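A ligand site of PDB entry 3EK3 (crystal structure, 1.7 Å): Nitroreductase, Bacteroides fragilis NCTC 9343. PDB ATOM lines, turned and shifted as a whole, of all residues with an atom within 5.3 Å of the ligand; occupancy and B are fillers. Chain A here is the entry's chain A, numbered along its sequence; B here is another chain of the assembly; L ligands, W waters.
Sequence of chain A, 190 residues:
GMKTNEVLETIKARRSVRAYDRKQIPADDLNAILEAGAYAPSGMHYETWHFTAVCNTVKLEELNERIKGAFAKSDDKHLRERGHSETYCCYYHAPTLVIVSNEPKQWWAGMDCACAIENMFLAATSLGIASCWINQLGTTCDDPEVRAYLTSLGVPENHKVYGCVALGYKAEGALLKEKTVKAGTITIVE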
ATOM      1  N   ARG A  14     -25.905 -25.693   8.042  1.00  0.00           N
ATOM      2  CA  ARG A  14     -25.729 -25.351   9.459  1.00  0.00           C
ATOM      3  C   ARG A  14     -24.858 -26.374  10.158  1.00  0.00           C
ATOM      4  O   ARG A  14     -25.165 -27.577  10.176  1.00  0.00           O
ATOM      5  CB  ARG A  14     -27.066 -25.240  10.181  1.00  0.00           C
ATOM      6  CG  ARG A  14     -26.963 -24.815  11.650  1.00  0.00           C
ATOM      7  CD  ARG A  14     -27.914 -25.558  12.562  1.00  0.00           C
ATOM      8  NE  ARG A  14     -27.844 -26.998  12.371  1.00  0.00           N
ATOM      9  CZ  ARG A  14     -26.894 -27.786  12.859  1.00  0.00           C
ATOM     10  NH1 ARG A  14     -25.921 -27.300  13.605  1.00  0.00           N
ATOM     11  NH2 ARG A  14     -26.904 -29.064  12.569  1.00  0.00           N
ATOM     12  N   ARG A  15     -23.782 -25.890  10.793  1.00  0.00           N
ATOM     13  CA  ARG A  15     -22.874 -26.774  11.520  1.00  0.00           C
ATOM     14  C   ARG A  15     -22.547 -26.198  12.881  1.00  0.00           C
ATOM     15  O   ARG A  15     -22.663 -24.985  13.123  1.00  0.00           O
ATOM     16  CB  ARG A  15     -21.578 -27.012  10.732  1.00  0.00           C
ATOM     17  CG  ARG A  15     -21.730 -27.726   9.374  1.00  0.00           C
ATOM     18  CD  ARG A  15     -22.334 -29.108   9.478  1.00  0.00           C
ATOM     19  NE  ARG A  15     -21.514 -30.016  10.282  1.00  0.00           N
ATOM     20  CZ  ARG A  15     -20.371 -30.568   9.881  1.00  0.00           C
ATOM     21  NH1 ARG A  15     -19.875 -30.309   8.665  1.00  0.00           N
ATOM     22  NH2 ARG A  15     -19.693 -31.380  10.712  1.00  0.00           N
ATOM     23  N   SER A  16     -22.105 -27.067  13.786  1.00  0.00           N
ATOM     24  CA  SER A  16     -21.597 -26.638  15.055  1.00  0.00           C
ATOM     25  C   SER A  16     -20.116 -26.279  14.948  1.00  0.00           C
ATOM     26  O   SER A  16     -19.256 -27.120  14.682  1.00  0.00           O
ATOM     27  CB  SER A  16     -21.777 -27.754  16.059  1.00  0.00           C
ATOM     28  OG  SER A  16     -23.152 -27.987  16.342  1.00  0.00           O
ATOM     29  N   ARG A  18     -16.624 -24.561  16.614  1.00  0.00           N
ATOM     30  CA  ARG A  18     -15.986 -24.521  17.938  1.00  0.00           C
ATOM     31  C   ARG A  18     -14.632 -23.836  17.913  1.00  0.00           C
ATOM     32  O   ARG A  18     -13.806 -24.039  18.788  1.00  0.00           O
ATOM     33  CB  ARG A  18     -15.859 -25.949  18.454  1.00  0.00           C
ATOM     34  CG  ARG A  18     -17.190 -26.710  18.456  1.00  0.00           C
ATOM     35  CD  ARG A  18     -17.100 -28.028  19.143  1.00  0.00           C
ATOM     36  NE  ARG A  18     -18.427 -28.636  19.241  1.00  0.00           N
ATOM     37  CZ  ARG A  18     -18.938 -29.527  18.409  1.00  0.00           C
ATOM     38  NH1 ARG A  18     -18.247 -29.955  17.381  1.00  0.00           N
ATOM     39  NH2 ARG A  18     -20.163 -29.999  18.620  1.00  0.00           N
ATOM     40  N   TYR A  92     -16.085 -21.648  23.617  1.00  0.00           N
ATOM     41  CA  TYR A  92     -15.061 -21.623  22.572  1.00  0.00           C
ATOM     42  C   TYR A  92     -14.563 -20.235  22.177  1.00  0.00           C
ATOM     43  O   TYR A  92     -14.152 -20.041  21.052  1.00  0.00           O
ATOM     44  CB  TYR A  92     -15.564 -22.388  21.332  1.00  0.00           C
ATOM     45  CG  TYR A  92     -16.087 -23.759  21.676  1.00  0.00           C
ATOM     46  CD1 TYR A  92     -15.236 -24.726  22.165  1.00  0.00           C
ATOM     47  CD2 TYR A  92     -17.415 -24.076  21.512  1.00  0.00           C
ATOM     48  CE1 TYR A  92     -15.708 -26.018  22.487  1.00  0.00           C
ATOM     49  CE2 TYR A  92     -17.906 -25.332  21.837  1.00  0.00           C
ATOM     50  CZ  TYR A  92     -17.057 -26.303  22.335  1.00  0.00           C
ATOM     51  OH  TYR A  92     -17.536 -27.566  22.636  1.00  0.00           O
ATOM     52  N   CYS A 132     -22.919 -22.453  17.645  1.00  0.00           N
ATOM     53  CA  CYS A 132     -22.898 -23.752  18.332  1.00  0.00           C
ATOM     54  C   CYS A 132     -23.812 -23.744  19.542  1.00  0.00           C
ATOM     55  O   CYS A 132     -23.892 -22.738  20.249  1.00  0.00           O
ATOM     56  CB  CYS A 132     -21.469 -24.063  18.790  1.00  0.00           C
ATOM     57  SG  CYS A 132     -21.110 -25.773  19.291  1.00  0.00           S
ATOM     58  N   TRP A 133     -24.470 -24.885  19.810  1.00  0.00           N
ATOM     59  CA  TRP A 133     -25.191 -25.112  21.046  1.00  0.00           C
ATOM     60  C   TRP A 133     -24.163 -25.235  22.154  1.00  0.00           C
ATOM     61  O   TRP A 133     -23.261 -26.054  22.061  1.00  0.00           O
ATOM     62  CB  TRP A 133     -26.008 -26.419  20.989  1.00  0.00           C
ATOM     63  CG  TRP A 133     -26.959 -26.577  22.114  1.00  0.00           C
ATOM     64  CD1 TRP A 133     -26.666 -26.761  23.429  1.00  0.00           C
ATOM     65  CD2 TRP A 133     -28.386 -26.633  22.017  1.00  0.00           C
ATOM     66  NE1 TRP A 133     -27.821 -26.873  24.157  1.00  0.00           N
ATOM     67  CE2 TRP A 133     -28.900 -26.826  23.319  1.00  0.00           C
ATOM     68  CE3 TRP A 133     -29.286 -26.551  20.940  1.00  0.00           C
ATOM     69  CZ2 TRP A 133     -30.263 -26.878  23.578  1.00  0.00           C
ATOM     70  CZ3 TRP A 133     -30.633 -26.628  21.190  1.00  0.00           C
ATOM     71  CH2 TRP A 133     -31.118 -26.820  22.507  1.00  0.00           C
ATOM     72  N   ILE A 134     -24.315 -24.435  23.199  1.00  0.00           N
ATOM     73  CA  ILE A 134     -23.524 -24.539  24.407  1.00  0.00           C
ATOM     74  C   ILE A 134     -24.473 -24.963  25.539  1.00  0.00           C
ATOM     75  O   ILE A 134     -25.363 -24.206  25.905  1.00  0.00           O
ATOM     76  CB  ILE A 134     -22.834 -23.183  24.704  1.00  0.00           C
ATOM     77  CG1 ILE A 134     -22.143 -22.629  23.421  1.00  0.00           C
ATOM     78  CG2 ILE A 134     -21.887 -23.306  25.869  1.00  0.00           C
ATOM     79  CD1 ILE A 134     -21.049 -23.589  22.852  1.00  0.00           C
ATOM     80  N   ASN A 135     -24.278 -26.192  26.048  1.00  0.00           N
ATOM     81  CA  ASN A 135     -25.216 -26.829  27.001  1.00  0.00           C
ATOM     82  C   ASN A 135     -24.821 -26.738  28.461  1.00  0.00           C
ATOM     83  O   ASN A 135     -25.543 -27.226  29.302  1.00  0.00           O
ATOM     84  CB  ASN A 135     -25.415 -28.294  26.617  1.00  0.00           C
ATOM     85  CG  ASN A 135     -26.828 -28.811  26.915  1.00  0.00           C
ATOM     86  OD1 ASN A 135     -27.810 -28.076  26.800  1.00  0.00           O
ATOM     87  ND2 ASN A 135     -26.914 -30.082  27.254  1.00  0.00           N
ATOM     88  N   GLN A 136     -23.694 -26.099  28.786  1.00  0.00           N
ATOM     89  CA  GLN A 136     -23.129 -26.250  30.120  1.00  0.00           C
ATOM     90  C   GLN A 136     -23.880 -25.499  31.218  1.00  0.00           C
ATOM     91  O   GLN A 136     -23.672 -25.784  32.394  1.00  0.00           O
ATOM     92  CB  GLN A 136     -21.642 -25.889  30.149  1.00  0.00           C
ATOM     93  CG  GLN A 136     -20.791 -26.940  29.502  1.00  0.00           C
ATOM     94  CD  GLN A 136     -21.083 -27.113  28.039  1.00  0.00           C
ATOM     95  OE1 GLN A 136     -21.061 -26.146  27.277  1.00  0.00           O
ATOM     96  NE2 GLN A 136     -21.343 -28.371  27.601  1.00  0.00           N
ATOM     97  N   LEU A 176     -14.129 -28.050   9.063  1.00  0.00           N
ATOM     98  CA  LEU A 176     -15.146 -28.935   9.652  1.00  0.00           C
ATOM     99  C   LEU A 176     -15.046 -30.329   9.040  1.00  0.00           C
ATOM    100  O   LEU A 176     -14.722 -30.464   7.869  1.00  0.00           O
ATOM    101  CB  LEU A 176     -16.555 -28.382   9.380  1.00  0.00           C
ATOM    102  CG  LEU A 176     -17.039 -27.159  10.170  1.00  0.00           C
ATOM    103  CD1 LEU A 176     -17.932 -26.280   9.320  1.00  0.00           C
ATOM    104  CD2 LEU A 176     -17.776 -27.582  11.431  1.00  0.00           C
ATOM    105  N   LYS A 179     -20.142 -33.466   6.699  1.00  0.00           N
ATOM    106  CA  LYS A 179     -21.366 -33.946   7.353  1.00  0.00           C
ATOM    107  C   LYS A 179     -22.085 -35.016   6.530  1.00  0.00           C
ATOM    108  O   LYS A 179     -22.357 -34.834   5.351  1.00  0.00           O
ATOM    109  CB  LYS A 179     -22.357 -32.828   7.689  1.00  0.00           C
ATOM    110  CG  LYS A 179     -23.688 -33.327   8.275  1.00  0.00           C
ATOM    111  CD  LYS A 179     -24.396 -32.283   9.116  1.00  0.00           C
ATOM    112  CE  LYS A 179     -25.574 -32.867   9.883  1.00  0.00           C
ATOM    113  NZ  LYS A 179     -26.256 -31.860  10.766  1.00  0.00           N
ATOM    114  N   TYR B  39     -31.078 -33.394   9.488  1.00  0.00           N
ATOM    115  CA  TYR B  39     -29.930 -32.493   9.563  1.00  0.00           C
ATOM    116  C   TYR B  39     -29.876 -31.546  10.773  1.00  0.00           C
ATOM    117  O   TYR B  39     -28.893 -30.795  10.954  1.00  0.00           O
ATOM    118  CB  TYR B  39     -29.829 -31.684   8.244  1.00  0.00           C
ATOM    119  CG  TYR B  39     -29.034 -32.382   7.178  1.00  0.00           C
ATOM    120  CD1 TYR B  39     -29.601 -33.373   6.380  1.00  0.00           C
ATOM    121  CD2 TYR B  39     -27.693 -32.078   6.980  1.00  0.00           C
ATOM    122  CE1 TYR B  39     -28.853 -34.025   5.408  1.00  0.00           C
ATOM    123  CE2 TYR B  39     -26.939 -32.734   6.030  1.00  0.00           C
ATOM    124  CZ  TYR B  39     -27.523 -33.706   5.250  1.00  0.00           C
ATOM    125  OH  TYR B  39     -26.787 -34.346   4.293  1.00  0.00           O
ATOM    126  N   ALA B  40     -30.885 -31.632  11.646  1.00  0.00           N
ATOM    127  CA  ALA B  40     -30.891 -30.909  12.908  1.00  0.00           C
ATOM    128  C   ALA B  40     -29.706 -31.326  13.807  1.00  0.00           C
ATOM    129  O   ALA B  40     -29.180 -32.451  13.741  1.00  0.00           O
ATOM    130  CB  ALA B  40     -32.263 -31.119  13.684  1.00  0.00           C
ATOM    131  N   PRO B  41     -29.284 -30.406  14.675  1.00  0.00           N
ATOM    132  CA  PRO B  41     -28.245 -30.742  15.604  1.00  0.00           C
ATOM    133  C   PRO B  41     -28.842 -31.716  16.609  1.00  0.00           C
ATOM    134  O   PRO B  41     -30.053 -31.665  16.861  1.00  0.00           O
ATOM    135  CB  PRO B  41     -27.931 -29.409  16.298  1.00  0.00           C
ATOM    136  CG  PRO B  41     -29.187 -28.580  16.157  1.00  0.00           C
ATOM    137  CD  PRO B  41     -29.760 -29.010  14.811  1.00  0.00           C
ATOM    138  N   SER B  42     -28.009 -32.610  17.109  1.00  0.00           N
ATOM    139  CA  SER B  42     -28.375 -33.485  18.248  1.00  0.00           C
ATOM    140  C   SER B  42     -27.237 -33.582  19.216  1.00  0.00           C
ATOM    141  O   SER B  42     -26.060 -33.570  18.845  1.00  0.00           O
ATOM    142  CB  SER B  42     -28.799 -34.891  17.784  1.00  0.00           C
ATOM    143  OG  SER B  42     -27.728 -35.638  17.212  1.00  0.00           O
ATOM    144  N   GLY B  43     -27.579 -33.732  20.506  1.00  0.00           N
ATOM    145  CA  GLY B  43     -26.559 -33.776  21.528  1.00  0.00           C
ATOM    146  C   GLY B  43     -25.628 -34.930  21.245  1.00  0.00           C
ATOM    147  O   GLY B  43     -26.102 -36.055  20.976  1.00  0.00           O
ATOM    148  N   MET B  44     -24.322 -34.644  21.291  1.00  0.00           N
ATOM    149  CA  MET B  44     -23.259 -35.656  21.061  1.00  0.00           C
ATOM    150  C   MET B  44     -23.309 -36.292  19.676  1.00  0.00           C
ATOM    151  O   MET B  44     -22.691 -37.355  19.439  1.00  0.00           O
ATOM    152  CB  MET B  44     -23.319 -36.729  22.158  1.00  0.00           C
ATOM    153  CG  MET B  44     -23.071 -36.176  23.541  1.00  0.00           C
ATOM    154  SD  MET B  44     -21.217 -35.668  23.779  1.00  0.00           S
ATOM    155  CE  MET B  44     -20.442 -37.377  23.466  1.00  0.00           C
ATOM    156  N   HIS B  45     -24.024 -35.652  18.736  1.00  0.00           N
ATOM    157  CA  HIS B  45     -24.330 -36.253  17.444  1.00  0.00           C
ATOM    158  C   HIS B  45     -24.877 -37.692  17.629  1.00  0.00           C
ATOM    159  O   HIS B  45     -24.623 -38.571  16.828  1.00  0.00           O
ATOM    160  CB  HIS B  45     -23.091 -36.217  16.534  1.00  0.00           C
ATOM    161  CG  HIS B  45     -23.384 -36.530  15.104  1.00  0.00           C
ATOM    162  ND1 HIS B  45     -24.454 -36.003  14.441  1.00  0.00           N
ATOM    163  CD2 HIS B  45     -22.783 -37.397  14.244  1.00  0.00           C
ATOM    164  CE1 HIS B  45     -24.486 -36.483  13.200  1.00  0.00           C
ATOM    165  NE2 HIS B  45     -23.491 -37.339  13.069  1.00  0.00           N
ATOM    166  N   TRP B 108     -31.680 -34.022  27.522  1.00  0.00           N
ATOM    167  CA  TRP B 108     -31.982 -33.152  26.401  1.00  0.00           C
ATOM    168  C   TRP B 108     -32.692 -33.867  25.236  1.00  0.00           C
ATOM    169  O   TRP B 108     -32.810 -33.298  24.129  1.00  0.00           O
ATOM    170  CB  TRP B 108     -30.690 -32.521  25.896  1.00  0.00           C
ATOM    171  CG  TRP B 108     -29.688 -33.526  25.415  1.00  0.00           C
ATOM    172  CD1 TRP B 108     -29.670 -34.148  24.203  1.00  0.00           C
ATOM    173  CD2 TRP B 108     -28.547 -34.002  26.134  1.00  0.00           C
ATOM    174  NE1 TRP B 108     -28.590 -35.011  24.136  1.00  0.00           N
ATOM    175  CE2 TRP B 108     -27.890 -34.933  25.307  1.00  0.00           C
ATOM    176  CE3 TRP B 108     -28.021 -33.724  27.401  1.00  0.00           C
ATOM    177  CZ2 TRP B 108     -26.713 -35.586  25.701  1.00  0.00           C
ATOM    178  CZ3 TRP B 108     -26.861 -34.360  27.789  1.00  0.00           C
ATOM    179  CH2 TRP B 108     -26.219 -35.291  26.937  1.00  0.00           C
ATOM    180  N   MET B 111     -35.172 -31.860  23.405  1.00  0.00           N
ATOM    181  CA  MET B 111     -34.632 -30.734  22.655  1.00  0.00           C
ATOM    182  C   MET B 111     -34.038 -31.176  21.339  1.00  0.00           C
ATOM    183  O   MET B 111     -34.200 -30.467  20.317  1.00  0.00           O
ATOM    184  CB  MET B 111     -33.641 -29.935  23.531  1.00  0.00           C
ATOM    185  CG  MET B 111     -34.296 -29.338  24.768  1.00  0.00           C
ATOM    186  SD  MET B 111     -33.275 -27.987  25.667  1.00  0.00           S
ATOM    187  CE  MET B 111     -31.713 -29.065  25.897  1.00  0.00           C
ATOM    188  N   ASP B 112     -33.383 -32.342  21.270  1.00  0.00           N
ATOM    189  CA  ASP B 112     -33.025 -32.873  19.946  1.00  0.00           C
ATOM    190  C   ASP B 112     -34.245 -32.833  19.018  1.00  0.00           C
ATOM    191  O   ASP B 112     -34.187 -32.373  17.906  1.00  0.00           O
ATOM    192  CB  ASP B 112     -32.585 -34.348  20.013  1.00  0.00           C
ATOM    193  CG  ASP B 112     -31.200 -34.572  20.596  1.00  0.00           C
ATOM    194  OD1 ASP B 112     -30.489 -33.625  20.979  1.00  0.00           O
ATOM    195  OD2 ASP B 112     -30.839 -35.767  20.652  1.00  0.00           O
ATOM    196  N   CYS B 115     -35.457 -29.486  17.823  1.00  0.00           N
ATOM    197  CA  CYS B 115     -34.606 -28.932  16.741  1.00  0.00           C
ATOM    198  C   CYS B 115     -34.978 -29.510  15.374  1.00  0.00           C
ATOM    199  O   CYS B 115     -35.071 -28.791  14.376  1.00  0.00           O
ATOM    200  CB  CYS B 115     -33.138 -29.156  17.011  1.00  0.00           C
ATOM    201  SG  CYS B 115     -32.460 -28.172  18.368  1.00  0.00           S
HETATM  202  N1  LIG L   1     -21.887 -28.851  21.094  1.00  0.00           N
HETATM  203  C1  LIG L   1     -20.921 -28.392  21.960  1.00  0.00           C
HETATM  204  O1  LIG L   1     -19.786 -28.127  21.547  1.00  0.00           O
HETATM  205  N2  LIG L   1     -21.158 -28.258  23.310  1.00  0.00           N
HETATM  206  C2  LIG L   1     -22.376 -28.584  23.805  1.00  0.00           C
HETATM  207  O2  LIG L   1     -22.620 -28.235  24.979  1.00  0.00           O
HETATM  208  C3  LIG L   1     -23.368 -29.032  22.930  1.00  0.00           C
HETATM  209  N3  LIG L   1     -24.612 -29.347  23.415  1.00  0.00           N
HETATM  210  C4  LIG L   1     -25.638 -29.755  22.577  1.00  0.00           C
HETATM  211  C5  LIG L   1     -26.894 -30.034  23.111  1.00  0.00           C
HETATM  212  C6  LIG L   1     -27.949 -30.416  22.283  1.00  0.00           C
HETATM  213  C7  LIG L   1     -29.376 -30.508  22.827  1.00  0.00           C
HETATM  214  C8  LIG L   1     -27.732 -30.488  20.903  1.00  0.00           C
HETATM  215  C9  LIG L   1     -28.925 -30.431  19.975  1.00  0.00           C
HETATM  216  C10 LIG L   1     -26.467 -30.205  20.372  1.00  0.00           C
HETATM  217  C11 LIG L   1     -25.401 -29.840  21.194  1.00  0.00           C
HETATM  218  N4  LIG L   1     -24.119 -29.573  20.703  1.00  0.00           N
HETATM  219  C12 LIG L   1     -23.136 -29.133  21.550  1.00  0.00           C
HETATM  220  C13 LIG L   1     -23.833 -29.637  19.224  1.00  0.00           C
HETATM  221  C14 LIG L   1     -23.780 -31.093  18.756  1.00  0.00           C
HETATM  222  O3  LIG L   1     -22.576 -31.700  19.175  1.00  0.00           O
HETATM  223  C15 LIG L   1     -23.833 -31.086  17.232  1.00  0.00           C
HETATM  224  O4  LIG L   1     -25.122 -30.662  16.848  1.00  0.00           O
HETATM  225  C16 LIG L   1     -23.602 -32.485  16.626  1.00  0.00           C
HETATM  226  O5  LIG L   1     -22.258 -32.900  16.854  1.00  0.00           O
HETATM  227  C17 LIG L   1     -23.884 -32.485  15.123  1.00  0.00           C
HETATM  228  O6  LIG L   1     -22.992 -31.602  14.461  1.00  0.00           O
HETATM  229  P1  LIG L   1     -23.514 -30.376  13.538  1.00  0.00           P
HETATM  230  O7  LIG L   1     -24.511 -30.924  12.592  1.00  0.00           O
HETATM  231  O8  LIG L   1     -22.286 -29.687  12.906  1.00  0.00           O
HETATM  232  O9  LIG L   1     -24.282 -29.420  14.406  1.00  0.00           O
HETATM  233  O   HOH W   1     -19.760 -29.823  13.764  1.00  0.00           O
HETATM  234  O   HOH W   2     -20.024 -31.768  15.912  1.00  0.00           O
HETATM  235  O   HOH W   3     -19.649 -26.538  24.955  1.00  0.00           O
HETATM  236  O   HOH W   4     -26.706 -34.528  14.934  1.00  0.00           O
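O1 of the ligand sits at hydrogen-bond distance from OH of Tyr 92 (2.6 Å).
The backbone NH (N) of Ser 16 sits at hydrogen-bond distance from an oxygen (O8) of the ligand.
O9 of the ligand sits at hydrogen-bond distance from OG of Ser 16 (2.7 Å).
The side-chain amino group (NZ) of Lys 179 lies within salt-bridge range of an oxygen (O7) of the ligand (2.7 Å).
NE of Arg 18 lies within hydrogen-bond range of O1 of the ligand (2.7 Å).
The guanidinium group (NE) of Arg 15 lies within salt-bridge range of an oxygen (O8) of the ligand (2.8 Å).
NH1 of Arg 14 lies within salt-bridge range of O9 of the ligand (2.8 Å).
N of Asn 135 sits at hydrogen-bond distance from O2 of the ligand.
NE2 of Gln 136 is in hydrogen-bond range of O2 of the ligand.
N2 of the ligand sits close to O of Trp 133, 3.3 Å away.
The backbone NH (N) of Ser 42 of chain B lies within hydrogen-bond range of an oxygen (O4) of the ligand, at 3.5 Å.
An oxygen (O1) of the ligand is in hydrogen-bond range of the side-chain sulfur (SG) of Cys 132 (3.5 Å).
O of Tyr 39 of chain B lies within hydrogen-bond range of NZ of Lys 179.
NH2 of Arg 14 sits at hydrogen-bond distance from O of Tyr 39 of chain B, 3.1 Å away.
OD1 of Asn 135 lies within hydrogen-bond range of NE1 of Trp 133.
OD1 of Asp 112 of chain B is in hydrogen-bond range of N of Gly 43 of chain B (3.0 Å).
Ile 134 touches the ligand (C to O2, 3.8 Å).
CB of Pro 41 of chain B touches O4 of the ligand, at 3.1 Å.
N of Gly 43 of chain B touches C8 of the ligand, 3.3 Å away.
His 45 of chain B touches the ligand.
CB of Trp 108 of chain B touches C7 of the ligand, 3.9 Å away.
OD1 of Asp 112 of chain B touches C9 of the ligand, at 3.7 Å.
Within 4 Å of the ligand: Arg 14, Arg 15, Ser 16, Arg 18, Tyr 92, Cys 132, Trp 133, Ile 134, Asn 135, Gln 136, Lys 179, Pro 41 of chain B, Ser 42 of chain B, Gly 43 of chain B, His 45 of chain B, Trp 108 of chain B and Asp 112 of chain B.
Water W1 lies within hydrogen-bond range of an oxygen (O8) of the ligand (2.7 Å), the backbone carbonyl oxygen (O) of Ser 16 (2.9 Å) and the guanidinium group (NH2) of Arg 15 (3.4 Å).
Water W2 lies within hydrogen-bond range of O5 of the ligand (2.7 Å) and NH1 of Arg 18 (2.9 Å).
Water W3 lies within hydrogen-bond range of OE1 of Gln 136 (2.7 Å), N2 of the ligand (2.8 Å) and OH of Tyr 92 (3.3 Å).
Water W4 lies within hydrogen-bond range of the side-chain hydroxyl (OG) of Ser 42 of chain B (2.7 Å), a ring nitrogen (ND1) of His 45 of chain B (2.7 Å) and the backbone carbonyl oxygen (O) of Ala 40 of chain B (3.4 Å).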
